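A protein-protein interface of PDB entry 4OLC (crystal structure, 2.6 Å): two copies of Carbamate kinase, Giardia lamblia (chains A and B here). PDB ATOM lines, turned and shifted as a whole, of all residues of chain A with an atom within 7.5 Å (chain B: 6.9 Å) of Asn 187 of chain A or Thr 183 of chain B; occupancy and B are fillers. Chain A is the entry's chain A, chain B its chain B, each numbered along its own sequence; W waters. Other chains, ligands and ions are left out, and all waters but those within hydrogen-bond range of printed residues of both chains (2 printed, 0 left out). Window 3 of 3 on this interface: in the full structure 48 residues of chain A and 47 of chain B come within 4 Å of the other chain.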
ATOM      1  N   SER A   3     -23.990  -2.517  11.918  1.00  0.00           N
ATOM      2  CA  SER A   3     -25.185  -2.310  12.728  1.00  0.00           C
ATOM      3  C   SER A   3     -26.318  -1.884  11.799  1.00  0.00           C
ATOM      4  O   SER A   3     -27.477  -2.273  11.983  1.00  0.00           O
ATOM      5  CB  SER A   3     -24.931  -1.245  13.800  1.00  0.00           C
ATOM      6  OG  SER A   3     -25.829  -1.382  14.892  1.00  0.00           O
ATOM      7  N   LYS A  49     -24.824  -7.754   7.096  1.00  0.00           N
ATOM      8  CA  LYS A  49     -24.893  -8.627   8.249  1.00  0.00           C
ATOM      9  C   LYS A  49     -25.034 -10.057   7.755  1.00  0.00           C
ATOM     10  O   LYS A  49     -25.999 -10.400   7.063  1.00  0.00           O
ATOM     11  CB  LYS A  49     -26.027  -8.212   9.190  1.00  0.00           C
ATOM     12  CG  LYS A  49     -25.531  -7.313  10.293  1.00  0.00           C
ATOM     13  CD  LYS A  49     -26.623  -6.441  10.863  1.00  0.00           C
ATOM     14  CE  LYS A  49     -27.934  -7.179  10.993  1.00  0.00           C
ATOM     15  NZ  LYS A  49     -28.821  -6.507  12.017  1.00  0.00           N
ATOM     16  N   ASN A 110     -15.201 -11.390  15.468  1.00  0.00           N
ATOM     17  CA  ASN A 110     -16.548 -11.317  16.034  1.00  0.00           C
ATOM     18  C   ASN A 110     -17.482 -12.259  15.277  1.00  0.00           C
ATOM     19  O   ASN A 110     -18.286 -11.825  14.445  1.00  0.00           O
ATOM     20  CB  ASN A 110     -17.087  -9.896  15.997  1.00  0.00           C
ATOM     21  CG  ASN A 110     -18.206  -9.671  17.002  1.00  0.00           C
ATOM     22  OD1 ASN A 110     -18.207 -10.241  18.097  1.00  0.00           O
ATOM     23  ND2 ASN A 110     -19.156  -8.827  16.639  1.00  0.00           N
ATOM     24  N   VAL A 180     -32.079 -17.109  19.204  1.00  0.00           N
ATOM     25  CA  VAL A 180     -30.742 -16.756  19.656  1.00  0.00           C
ATOM     26  C   VAL A 180     -29.889 -16.300  18.472  1.00  0.00           C
ATOM     27  O   VAL A 180     -29.004 -15.469  18.604  1.00  0.00           O
ATOM     28  CB  VAL A 180     -30.070 -17.950  20.359  1.00  0.00           C
ATOM     29  CG1 VAL A 180     -28.556 -17.717  20.515  1.00  0.00           C
ATOM     30  CG2 VAL A 180     -30.750 -18.214  21.703  1.00  0.00           C
ATOM     31  N   ILE A 181     -30.162 -16.875  17.309  1.00  0.00           N
ATOM     32  CA  ILE A 181     -29.513 -16.451  16.096  1.00  0.00           C
ATOM     33  C   ILE A 181     -29.872 -14.997  15.806  1.00  0.00           C
ATOM     34  O   ILE A 181     -29.019 -14.178  15.490  1.00  0.00           O
ATOM     35  CB  ILE A 181     -29.932 -17.370  14.946  1.00  0.00           C
ATOM     36  CG1 ILE A 181     -29.275 -18.737  15.142  1.00  0.00           C
ATOM     37  CG2 ILE A 181     -29.537 -16.773  13.600  1.00  0.00           C
ATOM     38  CD1 ILE A 181     -29.931 -19.829  14.376  1.00  0.00           C
ATOM     39  N   LYS A 182     -31.146 -14.678  15.947  1.00  0.00           N
ATOM     40  CA  LYS A 182     -31.616 -13.335  15.701  1.00  0.00           C
ATOM     41  C   LYS A 182     -31.032 -12.352  16.723  1.00  0.00           C
ATOM     42  O   LYS A 182     -30.683 -11.223  16.375  1.00  0.00           O
ATOM     43  CB  LYS A 182     -33.146 -13.315  15.665  1.00  0.00           C
ATOM     44  CG  LYS A 182     -33.770 -12.086  16.236  1.00  0.00           C
ATOM     45  CD  LYS A 182     -34.736 -11.445  15.249  1.00  0.00           C
ATOM     46  CE  LYS A 182     -35.568 -10.348  15.929  1.00  0.00           C
ATOM     47  NZ  LYS A 182     -34.747  -9.517  16.866  1.00  0.00           N
ATOM     48  N   THR A 183     -30.913 -12.780  17.978  1.00  0.00           N
ATOM     49  CA  THR A 183     -30.268 -11.958  18.989  1.00  0.00           C
ATOM     50  C   THR A 183     -28.847 -11.664  18.540  1.00  0.00           C
ATOM     51  O   THR A 183     -28.359 -10.544  18.692  1.00  0.00           O
ATOM     52  CB  THR A 183     -30.257 -12.644  20.392  1.00  0.00           C
ATOM     53  OG1 THR A 183     -31.569 -12.589  20.967  1.00  0.00           O
ATOM     54  CG2 THR A 183     -29.259 -11.959  21.348  1.00  0.00           C
ATOM     55  N   LEU A 184     -28.192 -12.669  17.972  1.00  0.00           N
ATOM     56  CA  LEU A 184     -26.821 -12.525  17.497  1.00  0.00           C
ATOM     57  C   LEU A 184     -26.610 -11.561  16.324  1.00  0.00           C
ATOM     58  O   LEU A 184     -25.736 -10.703  16.420  1.00  0.00           O
ATOM     59  CB  LEU A 184     -26.178 -13.877  17.204  1.00  0.00           C
ATOM     60  CG  LEU A 184     -25.795 -14.687  18.449  1.00  0.00           C
ATOM     61  CD1 LEU A 184     -25.342 -16.052  18.046  1.00  0.00           C
ATOM     62  CD2 LEU A 184     -24.731 -13.980  19.301  1.00  0.00           C
ATOM     63  N   ILE A 185     -27.359 -11.678  15.222  1.00  0.00           N
ATOM     64  CA  ILE A 185     -27.141 -10.702  14.140  1.00  0.00           C
ATOM     65  C   ILE A 185     -27.528  -9.288  14.586  1.00  0.00           C
ATOM     66  O   ILE A 185     -26.859  -8.318  14.236  1.00  0.00           O
ATOM     67  CB  ILE A 185     -27.814 -11.044  12.781  1.00  0.00           C
ATOM     68  CG1 ILE A 185     -29.171 -11.698  12.989  1.00  0.00           C
ATOM     69  CG2 ILE A 185     -26.930 -11.950  11.963  1.00  0.00           C
ATOM     70  CD1 ILE A 185     -30.025 -11.675  11.749  1.00  0.00           C
ATOM     71  N   ASP A 186     -28.598  -9.183  15.366  1.00  0.00           N
ATOM     72  CA  ASP A 186     -28.995  -7.909  15.945  1.00  0.00           C
ATOM     73  C   ASP A 186     -27.793  -7.267  16.617  1.00  0.00           C
ATOM     74  O   ASP A 186     -27.688  -6.037  16.693  1.00  0.00           O
ATOM     75  CB  ASP A 186     -30.125  -8.100  16.953  1.00  0.00           C
ATOM     76  CG  ASP A 186     -31.497  -8.279  16.287  1.00  0.00           C
ATOM     77  OD1 ASP A 186     -31.556  -8.341  15.032  1.00  0.00           O
ATOM     78  OD2 ASP A 186     -32.512  -8.364  17.022  1.00  0.00           O
ATOM     79  N   ASN A 187     -26.868  -8.095  17.087  1.00  0.00           N
ATOM     80  CA  ASN A 187     -25.697  -7.567  17.757  1.00  0.00           C
ATOM     81  C   ASN A 187     -24.462  -7.564  16.885  1.00  0.00           C
ATOM     82  O   ASN A 187     -23.352  -7.315  17.360  1.00  0.00           O
ATOM     83  CB  ASN A 187     -25.457  -8.273  19.090  1.00  0.00           C
ATOM     84  CG  ASN A 187     -26.465  -7.853  20.153  1.00  0.00           C
ATOM     85  OD1 ASN A 187     -26.220  -6.926  20.922  1.00  0.00           O
ATOM     86  ND2 ASN A 187     -27.608  -8.520  20.183  1.00  0.00           N
ATOM     87  N   ASN A 188     -24.665  -7.836  15.600  1.00  0.00           N
ATOM     88  CA  ASN A 188     -23.593  -7.704  14.621  1.00  0.00           C
ATOM     89  C   ASN A 188     -22.517  -8.772  14.716  1.00  0.00           C
ATOM     90  O   ASN A 188     -21.357  -8.531  14.352  1.00  0.00           O
ATOM     91  CB  ASN A 188     -22.922  -6.338  14.761  1.00  0.00           C
ATOM     92  CG  ASN A 188     -23.662  -5.262  14.045  1.00  0.00           C
ATOM     93  OD1 ASN A 188     -24.605  -4.667  14.588  1.00  0.00           O
ATOM     94  ND2 ASN A 188     -23.255  -5.001  12.805  1.00  0.00           N
ATOM     95  N   VAL A 189     -22.901  -9.932  15.230  1.00  0.00           N
ATOM     96  CA  VAL A 189     -22.019 -11.085  15.238  1.00  0.00           C
ATOM     97  C   VAL A 189     -22.228 -11.835  13.940  1.00  0.00           C
ATOM     98  O   VAL A 189     -23.372 -12.099  13.545  1.00  0.00           O
ATOM     99  CB  VAL A 189     -22.329 -11.999  16.441  1.00  0.00           C
ATOM    100  CG1 VAL A 189     -21.431 -13.245  16.436  1.00  0.00           C
ATOM    101  CG2 VAL A 189     -22.172 -11.210  17.730  1.00  0.00           C
ATOM    102  N   LEU A 190     -21.134 -12.151  13.259  1.00  0.00           N
ATOM    103  CA  LEU A 190     -21.227 -12.992  12.075  1.00  0.00           C
ATOM    104  C   LEU A 190     -21.518 -14.438  12.547  1.00  0.00           C
ATOM    105  O   LEU A 190     -20.677 -15.097  13.148  1.00  0.00           O
ATOM    106  CB  LEU A 190     -19.972 -12.845  11.200  1.00  0.00           C
ATOM    107  CG  LEU A 190     -19.377 -13.991  10.339  1.00  0.00           C
ATOM    108  CD1 LEU A 190     -20.227 -15.265  10.224  1.00  0.00           C
ATOM    109  CD2 LEU A 190     -18.962 -13.495   8.939  1.00  0.00           C
ATOM    110  N   TYR B 178     -14.838 -15.168  23.579  1.00  0.00           N
ATOM    111  CA  TYR B 178     -15.224 -14.395  24.765  1.00  0.00           C
ATOM    112  C   TYR B 178     -16.265 -13.281  24.505  1.00  0.00           C
ATOM    113  O   TYR B 178     -17.282 -13.201  25.197  1.00  0.00           O
ATOM    114  CB  TYR B 178     -13.996 -13.794  25.454  1.00  0.00           C
ATOM    115  CG  TYR B 178     -14.398 -12.641  26.331  1.00  0.00           C
ATOM    116  CD1 TYR B 178     -14.992 -12.865  27.573  1.00  0.00           C
ATOM    117  CD2 TYR B 178     -14.233 -11.320  25.909  1.00  0.00           C
ATOM    118  CE1 TYR B 178     -15.388 -11.807  28.369  1.00  0.00           C
ATOM    119  CE2 TYR B 178     -14.634 -10.269  26.696  1.00  0.00           C
ATOM    120  CZ  TYR B 178     -15.214 -10.514  27.929  1.00  0.00           C
ATOM    121  OH  TYR B 178     -15.617  -9.466  28.745  1.00  0.00           O
ATOM    122  N   GLY B 179     -16.007 -12.423  23.525  1.00  0.00           N
ATOM    123  CA  GLY B 179     -16.904 -11.326  23.223  1.00  0.00           C
ATOM    124  C   GLY B 179     -18.342 -11.711  22.881  1.00  0.00           C
ATOM    125  O   GLY B 179     -19.293 -10.999  23.233  1.00  0.00           O
ATOM    126  N   VAL B 180     -18.519 -12.825  22.178  1.00  0.00           N
ATOM    127  CA  VAL B 180     -19.862 -13.236  21.795  1.00  0.00           C
ATOM    128  C   VAL B 180     -20.580 -13.811  23.013  1.00  0.00           C
ATOM    129  O   VAL B 180     -21.783 -13.618  23.202  1.00  0.00           O
ATOM    130  CB  VAL B 180     -19.836 -14.304  20.675  1.00  0.00           C
ATOM    131  CG1 VAL B 180     -21.255 -14.775  20.349  1.00  0.00           C
ATOM    132  CG2 VAL B 180     -19.113 -13.789  19.432  1.00  0.00           C
ATOM    133  N   ILE B 181     -19.842 -14.537  23.842  1.00  0.00           N
ATOM    134  CA  ILE B 181     -20.453 -15.144  25.014  1.00  0.00           C
ATOM    135  C   ILE B 181     -21.004 -14.034  25.894  1.00  0.00           C
ATOM    136  O   ILE B 181     -22.139 -14.101  26.345  1.00  0.00           O
ATOM    137  CB  ILE B 181     -19.458 -16.034  25.774  1.00  0.00           C
ATOM    138  CG1 ILE B 181     -18.903 -17.097  24.821  1.00  0.00           C
ATOM    139  CG2 ILE B 181     -20.129 -16.683  26.965  1.00  0.00           C
ATOM    140  CD1 ILE B 181     -17.853 -18.023  25.431  1.00  0.00           C
ATOM    141  N   LYS B 182     -20.195 -13.001  26.100  1.00  0.00           N
ATOM    142  CA  LYS B 182     -20.568 -11.862  26.920  1.00  0.00           C
ATOM    143  C   LYS B 182     -21.854 -11.240  26.390  1.00  0.00           C
ATOM    144  O   LYS B 182     -22.751 -10.883  27.146  1.00  0.00           O
ATOM    145  CB  LYS B 182     -19.436 -10.833  26.896  1.00  0.00           C
ATOM    146  CG  LYS B 182     -19.768  -9.504  27.522  1.00  0.00           C
ATOM    147  CD  LYS B 182     -19.996  -9.638  29.013  1.00  0.00           C
ATOM    148  CE  LYS B 182     -19.958  -8.291  29.723  1.00  0.00           C
ATOM    149  NZ  LYS B 182     -21.099  -7.407  29.316  1.00  0.00           N
ATOM    150  N   THR B 183     -21.928 -11.122  25.069  1.00  0.00           N
ATOM    151  CA  THR B 183     -23.084 -10.558  24.420  1.00  0.00           C
ATOM    152  C   THR B 183     -24.301 -11.390  24.751  1.00  0.00           C
ATOM    153  O   THR B 183     -25.329 -10.855  25.153  1.00  0.00           O
ATOM    154  CB  THR B 183     -22.864 -10.468  22.885  1.00  0.00           C
ATOM    155  OG1 THR B 183     -21.909  -9.437  22.596  1.00  0.00           O
ATOM    156  CG2 THR B 183     -24.157 -10.154  22.144  1.00  0.00           C
ATOM    157  N   LEU B 184     -24.172 -12.704  24.602  1.00  0.00           N
ATOM    158  CA  LEU B 184     -25.277 -13.629  24.864  1.00  0.00           C
ATOM    159  C   LEU B 184     -25.793 -13.598  26.304  1.00  0.00           C
ATOM    160  O   LEU B 184     -27.011 -13.666  26.502  1.00  0.00           O
ATOM    161  CB  LEU B 184     -24.953 -15.070  24.410  1.00  0.00           C
ATOM    162  CG  LEU B 184     -24.931 -15.393  22.904  1.00  0.00           C
ATOM    163  CD1 LEU B 184     -24.522 -16.848  22.655  1.00  0.00           C
ATOM    164  CD2 LEU B 184     -26.262 -15.135  22.255  1.00  0.00           C
ATOM    165  N   ILE B 185     -24.922 -13.504  27.312  1.00  0.00           N
ATOM    166  CA  ILE B 185     -25.467 -13.396  28.671  1.00  0.00           C
ATOM    167  C   ILE B 185     -26.047 -12.005  28.972  1.00  0.00           C
ATOM    168  O   ILE B 185     -27.056 -11.886  29.674  1.00  0.00           O
ATOM    169  CB  ILE B 185     -24.522 -13.870  29.804  1.00  0.00           C
ATOM    170  CG1 ILE B 185     -23.145 -13.244  29.684  1.00  0.00           C
ATOM    171  CG2 ILE B 185     -24.420 -15.391  29.811  1.00  0.00           C
ATOM    172  CD1 ILE B 185     -22.090 -13.989  30.517  1.00  0.00           C
ATOM    173  N   ASP B 186     -25.434 -10.964  28.421  1.00  0.00           N
ATOM    174  CA  ASP B 186     -26.010  -9.637  28.563  1.00  0.00           C
ATOM    175  C   ASP B 186     -27.464  -9.688  28.128  1.00  0.00           C
ATOM    176  O   ASP B 186     -28.294  -9.009  28.700  1.00  0.00           O
ATOM    177  CB  ASP B 186     -25.238  -8.596  27.759  1.00  0.00           C
ATOM    178  CG  ASP B 186     -23.842  -8.373  28.291  1.00  0.00           C
ATOM    179  OD1 ASP B 186     -23.539  -8.877  29.402  1.00  0.00           O
ATOM    180  OD2 ASP B 186     -23.049  -7.688  27.600  1.00  0.00           O
ATOM    181  N   ASN B 187     -27.761 -10.522  27.141  1.00  0.00           N
ATOM    182  CA  ASN B 187     -29.124 -10.697  26.650  1.00  0.00           C
ATOM    183  C   ASN B 187     -29.892 -11.845  27.313  1.00  0.00           C
ATOM    184  O   ASN B 187     -30.977 -12.222  26.864  1.00  0.00           O
ATOM    185  CB  ASN B 187     -29.124 -10.919  25.137  1.00  0.00           C
ATOM    186  CG  ASN B 187     -28.802  -9.658  24.356  1.00  0.00           C
ATOM    187  OD1 ASN B 187     -29.700  -8.907  23.995  1.00  0.00           O
ATOM    188  ND2 ASN B 187     -27.519  -9.425  24.089  1.00  0.00           N
ATOM    189  N   ASN B 188     -29.335 -12.423  28.367  1.00  0.00           N
ATOM    190  CA  ASN B 188     -30.064 -13.445  29.093  1.00  0.00           C
ATOM    191  C   ASN B 188     -30.237 -14.763  28.371  1.00  0.00           C
ATOM    192  O   ASN B 188     -31.207 -15.480  28.614  1.00  0.00           O
ATOM    193  CB  ASN B 188     -31.442 -12.930  29.475  1.00  0.00           C
ATOM    194  CG  ASN B 188     -31.665 -12.972  30.971  1.00  0.00           C
ATOM    195  OD1 ASN B 188     -31.199 -12.085  31.683  1.00  0.00           O
ATOM    196  ND2 ASN B 188     -32.356 -14.014  31.461  1.00  0.00           N
ATOM    197  N   VAL B 189     -29.316 -15.088  27.476  1.00  0.00           N
ATOM    198  CA  VAL B 189     -29.300 -16.423  26.918  1.00  0.00           C
ATOM    199  C   VAL B 189     -28.542 -17.347  27.859  1.00  0.00           C
ATOM    200  O   VAL B 189     -27.492 -16.996  28.374  1.00  0.00           O
ATOM    201  CB  VAL B 189     -28.669 -16.441  25.533  1.00  0.00           C
ATOM    202  CG1 VAL B 189     -28.737 -17.852  24.938  1.00  0.00           C
ATOM    203  CG2 VAL B 189     -29.399 -15.466  24.652  1.00  0.00           C
ATOM    204  N   VAL B 191     -26.102 -19.717  28.036  1.00  0.00           N
ATOM    205  CA  VAL B 191     -25.033 -20.095  27.127  1.00  0.00           C
ATOM    206  C   VAL B 191     -24.332 -21.394  27.543  1.00  0.00           C
ATOM    207  O   VAL B 191     -23.885 -21.535  28.692  1.00  0.00           O
ATOM    208  CB  VAL B 191     -23.951 -18.995  27.043  1.00  0.00           C
ATOM    209  CG1 VAL B 191     -22.908 -19.357  25.999  1.00  0.00           C
ATOM    210  CG2 VAL B 191     -24.593 -17.645  26.719  1.00  0.00           C
ATOM    211  N   LEU B 228     -15.334 -12.594  32.140  1.00  0.00           N
ATOM    212  CA  LEU B 228     -16.722 -12.173  32.035  1.00  0.00           C
ATOM    213  C   LEU B 228     -17.069 -11.352  33.267  1.00  0.00           C
ATOM    214  O   LEU B 228     -18.182 -10.832  33.397  1.00  0.00           O
ATOM    215  CB  LEU B 228     -17.612 -13.413  32.022  1.00  0.00           C
ATOM    216  CG  LEU B 228     -18.445 -13.858  30.830  1.00  0.00           C
ATOM    217  CD1 LEU B 228     -17.848 -13.410  29.523  1.00  0.00           C
ATOM    218  CD2 LEU B 228     -18.594 -15.380  30.871  1.00  0.00           C
HETATM  219  O   HOH W   1     -30.602  -7.659  21.313  1.00  0.00           O
HETATM  220  O   HOH W   2     -26.085  -7.264  23.518  1.00  0.00           O
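The backbone carbonyl oxygen (O) of Thr 183 of chain B lies within hydrogen-bond range of the side-chain amide nitrogen (ND2) of Asn 187 of chain B (2.8 Å).
N of Leu 190 of chain A lies within hydrogen-bond range of O of Asn 110 of chain A (3.1 Å).
N of Val 189 of chain B lies within hydrogen-bond range of O of Leu 184 of chain B, 2.9 Å away.
O of Thr 183 of chain A sits at hydrogen-bond distance from ND2 of Asn 187 of chain A, at 2.6 Å.
O of Asn 188 of chain A sits at hydrogen-bond distance from ND2 of Asn 110 of chain A (3.2 Å).
The backbone carbonyl oxygen (O) of Leu 184 of chain A lies within hydrogen-bond range of the backbone NH (N) of Val 189 of chain A (3.2 Å).
Asn 110 of chain A touches Val 180 of chain B (OD1 to CG2, 3.9 Å).
Leu 184 of chain B touches Val 180 of chain A (CD2 to CG1, 3.9 Å).
CG2 of Val 180 of chain A touches CG1 of Val 189 of chain B, 3.8 Å away.
CG2 of Thr 183 of chain A touches CG of Asn 187 of chain B (3.8 Å).
CD2 of Leu 184 of chain A touches CG1 of Val 180 of chain B, 3.7 Å away.
CD2 of Leu 184 of chain A touches CD2 of Leu 184 of chain B, 3.5 Å away.
CB of Asn 187 of chain A touches CG2 of Thr 183 of chain B (3.8 Å).
Val 189 of chain A touches Val 180 of chain B (CG1 to CG2, 3.8 Å).
Of the printed residues of chain B, Asn 187 of chain A touches Thr 183.
Of chain A, only Asn 187 comes within 4 Å of Thr 183 of chain B.
Printed residues of chain B within 4 Å of Val 180 of chain A: Leu 184 (3.9 Å) and Val 189 (3.8 Å).
Printed residues of chain A within 4 Å of Val 189 of chain B: Val 180.
Leu 190 of chain A touches none of the printed residues of chain B.
The nearest printed residue of chain B that does not touch Asn 187 of chain A is Asn 187 of chain B (4.01 Å).
The nearest residue of chain A that does not touch Thr 183 of chain B is Leu 184 of chain A (4.8 Å).
Of the 14 printed residues of chain B, 5 touch a printed residue of chain A.
Among the printed residues, 8 pairs touch across the chains.
Among the printed residues, no Asp or Glu carboxylate lies within 4 Å of a Lys or Arg side-chain nitrogen of the other chain.
Val 180 of chain A touches Leu 184 of chain B, and with the chains exchanged Leu 184 of chain A touches Val 180 of chain B.
Val 180 of chain A touches Val 189 of chain B, and with the chains exchanged Val 189 of chain A touches Val 180 of chain B.
Thr 183 of chain A touches Asn 187 of chain B, and with the chains exchanged Asn 187 of chain A touches Thr 183 of chain B.
Leu 184 of chain B touches its own counterpart, Leu 184 of chain A.
Positions printed for both chains: 180, 181, 182, 183, 184, 185, 186, 187, 188 and 189.
Water W2 lies within hydrogen-bond range of OD1 of Asn 187 of chain A (2.6 Å) and ND2 of Asn 187 of chain B (2.7 Å).
Water W1 bridges OD1 of Asn 187 of chain B (3.1 Å) and ND2 of Asn 187 of chain A (3.3 Å).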
